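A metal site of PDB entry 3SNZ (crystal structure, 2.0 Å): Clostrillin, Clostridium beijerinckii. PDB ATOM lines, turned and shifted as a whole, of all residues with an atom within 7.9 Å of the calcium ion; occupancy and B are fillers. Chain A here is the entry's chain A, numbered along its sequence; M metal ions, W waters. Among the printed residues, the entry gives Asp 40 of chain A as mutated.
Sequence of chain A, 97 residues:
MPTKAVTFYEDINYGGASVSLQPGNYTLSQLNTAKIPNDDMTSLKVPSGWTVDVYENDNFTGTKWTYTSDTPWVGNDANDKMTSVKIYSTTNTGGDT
The calcium ion is bound by O of Glu 10, OD1 of Asp 80, O of Asp 40, OG1 of Thr 42 and water W1.
Within 4 Å of the calcium ion: Glu 10, Asp 40, Thr 42 and Asp 80.
N of Asp 80 is in hydrogen-bond range of O of Met 41.
The side-chain carboxylate (OD1) of Asp 80 lies close to the side-chain amide oxygen (OD1) of Asn 79, 3.4 Å away.
OG1 of Thr 42 sits close to OD1 of Asn 79 (2.7 Å).
N of Thr 42 sits at hydrogen-bond distance from O of Tyr 9 (3.0 Å).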
ATOM      1  N   TYR A   9       3.227  21.622  -6.002  1.00  0.00           N
ATOM      2  CA  TYR A   9       2.987  21.109  -4.646  1.00  0.00           C
ATOM      3  C   TYR A   9       2.975  19.582  -4.671  1.00  0.00           C
ATOM      4  O   TYR A   9       2.523  18.982  -5.639  1.00  0.00           O
ATOM      5  CB  TYR A   9       1.672  21.649  -4.084  1.00  0.00           C
ATOM      6  CG  TYR A   9       1.679  23.147  -3.871  1.00  0.00           C
ATOM      7  CD1 TYR A   9       2.042  23.687  -2.631  1.00  0.00           C
ATOM      8  CD2 TYR A   9       1.329  24.019  -4.898  1.00  0.00           C
ATOM      9  CE1 TYR A   9       2.053  25.075  -2.429  1.00  0.00           C
ATOM     10  CE2 TYR A   9       1.352  25.398  -4.716  1.00  0.00           C
ATOM     11  CZ  TYR A   9       1.707  25.914  -3.473  1.00  0.00           C
ATOM     12  OH  TYR A   9       1.731  27.281  -3.284  1.00  0.00           O
ATOM     13  N   GLU A  10       3.436  18.978  -3.573  1.00  0.00           N
ATOM     14  CA  GLU A  10       3.560  17.531  -3.476  1.00  0.00           C
ATOM     15  C   GLU A  10       2.265  16.814  -3.110  1.00  0.00           C
ATOM     16  O   GLU A  10       2.075  15.652  -3.456  1.00  0.00           O
ATOM     17  CB  GLU A  10       4.691  17.130  -2.514  1.00  0.00           C
ATOM     18  CG  GLU A  10       6.088  17.397  -3.120  1.00  0.00           C
ATOM     19  CD  GLU A  10       7.246  16.858  -2.271  1.00  0.00           C
ATOM     20  OE1 GLU A  10       7.017  15.951  -1.436  1.00  0.00           O
ATOM     21  OE2 GLU A  10       8.383  17.347  -2.461  1.00  0.00           O
ATOM     22  N   ASP A  11       1.368  17.488  -2.398  1.00  0.00           N
ATOM     23  CA  ASP A  11       0.043  16.918  -2.175  1.00  0.00           C
ATOM     24  C   ASP A  11      -1.085  17.793  -2.740  1.00  0.00           C
ATOM     25  O   ASP A  11      -0.853  18.906  -3.217  1.00  0.00           O
ATOM     26  CB  ASP A  11      -0.202  16.559  -0.696  1.00  0.00           C
ATOM     27  CG  ASP A  11      -1.371  15.575  -0.499  1.00  0.00           C
ATOM     28  OD1 ASP A  11      -1.629  14.701  -1.368  1.00  0.00           O
ATOM     29  OD2 ASP A  11      -2.057  15.685   0.534  1.00  0.00           O
ATOM     30  N   ILE A  12      -2.281  17.229  -2.686  1.00  0.00           N
ATOM     31  CA  ILE A  12      -3.521  17.821  -3.153  1.00  0.00           C
ATOM     32  C   ILE A  12      -3.793  19.179  -2.465  1.00  0.00           C
ATOM     33  O   ILE A  12      -3.241  19.474  -1.403  1.00  0.00           O
ATOM     34  CB  ILE A  12      -4.671  16.767  -2.910  1.00  0.00           C
ATOM     35  CG1 ILE A  12      -5.623  16.663  -4.115  1.00  0.00           C
ATOM     36  CG2 ILE A  12      -5.364  16.968  -1.537  1.00  0.00           C
ATOM     37  CD1 ILE A  12      -6.797  17.626  -4.070  1.00  0.00           C
ATOM     38  N   GLY A  15      -1.089  21.507  -0.699  1.00  0.00           N
ATOM     39  CA  GLY A  15      -0.465  21.054   0.548  1.00  0.00           C
ATOM     40  C   GLY A  15       0.891  20.412   0.332  1.00  0.00           C
ATOM     41  O   GLY A  15       1.250  20.048  -0.786  1.00  0.00           O
ATOM     42  N   ASN A  38      11.264  13.333  -8.645  1.00  0.00           N
ATOM     43  CA  ASN A  38      10.559  12.640  -9.702  1.00  0.00           C
ATOM     44  C   ASN A  38       9.171  12.170  -9.239  1.00  0.00           C
ATOM     45  O   ASN A  38       8.993  11.779  -8.083  1.00  0.00           O
ATOM     46  CB  ASN A  38      11.375  11.440 -10.145  1.00  0.00           C
ATOM     47  CG  ASN A  38      10.943  10.892 -11.486  1.00  0.00           C
ATOM     48  OD1 ASN A  38      10.313  11.590 -12.282  1.00  0.00           O
ATOM     49  ND2 ASN A  38      11.269   9.652 -11.742  1.00  0.00           N
ATOM     50  N   ASP A  39       8.199  12.222 -10.148  1.00  0.00           N
ATOM     51  CA  ASP A  39       6.871  11.609  -9.948  1.00  0.00           C
ATOM     52  C   ASP A  39       6.201  11.990  -8.629  1.00  0.00           C
ATOM     53  O   ASP A  39       5.687  11.116  -7.913  1.00  0.00           O
ATOM     54  CB  ASP A  39       6.984  10.087 -10.049  1.00  0.00           C
ATOM     55  CG  ASP A  39       7.432   9.631 -11.426  1.00  0.00           C
ATOM     56  OD1 ASP A  39       7.238  10.392 -12.391  1.00  0.00           O
ATOM     57  OD2 ASP A  39       7.968   8.502 -11.540  1.00  0.00           O
ATOM     58  N   ASP A  40       6.184  13.283  -8.303  1.00  0.00           N
ATOM     59  CA  ASP A  40       5.744  13.698  -6.974  1.00  0.00           C
ATOM     60  C   ASP A  40       4.781  14.888  -6.975  1.00  0.00           C
ATOM     61  O   ASP A  40       4.316  15.313  -5.911  1.00  0.00           O
ATOM     62  CB  ASP A  40       6.963  13.995  -6.112  1.00  0.00           C
ATOM     63  CG  ASP A  40       6.701  13.860  -4.614  1.00  0.00           C
ATOM     64  OD1 ASP A  40       5.728  13.180  -4.183  1.00  0.00           O
ATOM     65  OD2 ASP A  40       7.491  14.442  -3.851  1.00  0.00           O
ATOM     66  N   MET A  41       4.465  15.393  -8.153  1.00  0.00           N
ATOM     67  CA  MET A  41       3.641  16.596  -8.248  1.00  0.00           C
ATOM     68  C   MET A  41       2.156  16.228  -8.296  1.00  0.00           C
ATOM     69  O   MET A  41       1.727  15.423  -9.123  1.00  0.00           O
ATOM     70  CB  MET A  41       4.074  17.440  -9.451  1.00  0.00           C
ATOM     71  CG  MET A  41       3.524  18.836  -9.467  1.00  0.00           C
ATOM     72  SD  MET A  41       1.884  18.924 -10.196  1.00  0.00           S
ATOM     73  CE  MET A  41       2.197  18.538 -11.925  1.00  0.00           C
ATOM     74  N   THR A  42       1.382  16.845  -7.398  1.00  0.00           N
ATOM     75  CA  THR A  42      -0.058  16.569  -7.261  1.00  0.00           C
ATOM     76  C   THR A  42      -0.943  17.787  -7.504  1.00  0.00           C
ATOM     77  O   THR A  42      -2.071  17.649  -7.983  1.00  0.00           O
ATOM     78  CB  THR A  42      -0.380  15.960  -5.866  1.00  0.00           C
ATOM     79  OG1 THR A  42       0.351  14.730  -5.722  1.00  0.00           O
ATOM     80  CG2 THR A  42      -1.861  15.672  -5.717  1.00  0.00           C
ATOM     81  N   SER A  43      -0.442  18.985  -7.182  1.00  0.00           N
ATOM     82  CA  SER A  43      -1.153  20.214  -7.511  1.00  0.00           C
ATOM     83  C   SER A  43      -0.171  21.315  -7.860  1.00  0.00           C
ATOM     84  O   SER A  43       1.014  21.238  -7.535  1.00  0.00           O
ATOM     85  CB  SER A  43      -2.075  20.622  -6.345  1.00  0.00           C
ATOM     86  OG  SER A  43      -1.362  21.042  -5.199  1.00  0.00           O
ATOM     87  N   TRP A  73      -5.876  19.817  -7.953  1.00  0.00           N
ATOM     88  CA  TRP A  73      -5.821  18.371  -8.133  1.00  0.00           C
ATOM     89  C   TRP A  73      -5.613  18.040  -9.614  1.00  0.00           C
ATOM     90  O   TRP A  73      -6.451  18.387 -10.447  1.00  0.00           O
ATOM     91  CB  TRP A  73      -7.116  17.755  -7.593  1.00  0.00           C
ATOM     92  CG  TRP A  73      -7.362  16.317  -7.910  1.00  0.00           C
ATOM     93  CD1 TRP A  73      -8.522  15.784  -8.378  1.00  0.00           C
ATOM     94  CD2 TRP A  73      -6.437  15.221  -7.759  1.00  0.00           C
ATOM     95  NE1 TRP A  73      -8.379  14.428  -8.549  1.00  0.00           N
ATOM     96  CE2 TRP A  73      -7.119  14.062  -8.171  1.00  0.00           C
ATOM     97  CE3 TRP A  73      -5.117  15.108  -7.319  1.00  0.00           C
ATOM     98  CZ2 TRP A  73      -6.520  12.800  -8.164  1.00  0.00           C
ATOM     99  CZ3 TRP A  73      -4.526  13.865  -7.321  1.00  0.00           C
ATOM    100  CH2 TRP A  73      -5.222  12.718  -7.738  1.00  0.00           C
ATOM    101  N   ASN A  79      -1.480  12.421 -11.856  1.00  0.00           N
ATOM    102  CA  ASN A  79      -0.929  12.545 -10.496  1.00  0.00           C
ATOM    103  C   ASN A  79       0.394  11.808 -10.327  1.00  0.00           C
ATOM    104  O   ASN A  79       0.533  10.668 -10.784  1.00  0.00           O
ATOM    105  CB  ASN A  79      -1.925  12.048  -9.442  1.00  0.00           C
ATOM    106  CG  ASN A  79      -1.515  12.408  -8.031  1.00  0.00           C
ATOM    107  OD1 ASN A  79      -0.718  13.334  -7.830  1.00  0.00           O
ATOM    108  ND2 ASN A  79      -2.043  11.686  -7.041  1.00  0.00           N
ATOM    109  N   ASP A  80       1.363  12.458  -9.680  1.00  0.00           N
ATOM    110  CA  ASP A  80       2.692  11.860  -9.414  1.00  0.00           C
ATOM    111  C   ASP A  80       3.388  11.308 -10.680  1.00  0.00           C
ATOM    112  O   ASP A  80       4.002  10.238 -10.630  1.00  0.00           O
ATOM    113  CB  ASP A  80       2.570  10.779  -8.328  1.00  0.00           C
ATOM    114  CG  ASP A  80       2.192  11.370  -6.976  1.00  0.00           C
ATOM    115  OD1 ASP A  80       2.390  12.583  -6.806  1.00  0.00           O
ATOM    116  OD2 ASP A  80       1.692  10.621  -6.100  1.00  0.00           O
ATOM    117  N   LYS A  81       3.291  12.049 -11.783  1.00  0.00           N
ATOM    118  CA  LYS A  81       3.865  11.635 -13.062  1.00  0.00           C
ATOM    119  C   LYS A  81       4.895  12.594 -13.638  1.00  0.00           C
ATOM    120  O   LYS A  81       5.556  12.270 -14.621  1.00  0.00           O
ATOM    121  CB  LYS A  81       2.772  11.395 -14.118  1.00  0.00           C
ATOM    122  CG  LYS A  81       1.826  10.218 -13.824  1.00  0.00           C
ATOM    123  CD  LYS A  81       2.563   8.886 -13.798  1.00  0.00           C
ATOM    124  CE  LYS A  81       1.713   7.757 -14.363  1.00  0.00           C
ATOM    125  NZ  LYS A  81       0.380   7.705 -13.721  1.00  0.00           N
HETATM  126 CA    CA M   1       2.658  13.773  -4.704  1.00  0.00          CA
HETATM  127  O   HOH W   1       0.718  12.178  -3.694  1.00  0.00           O
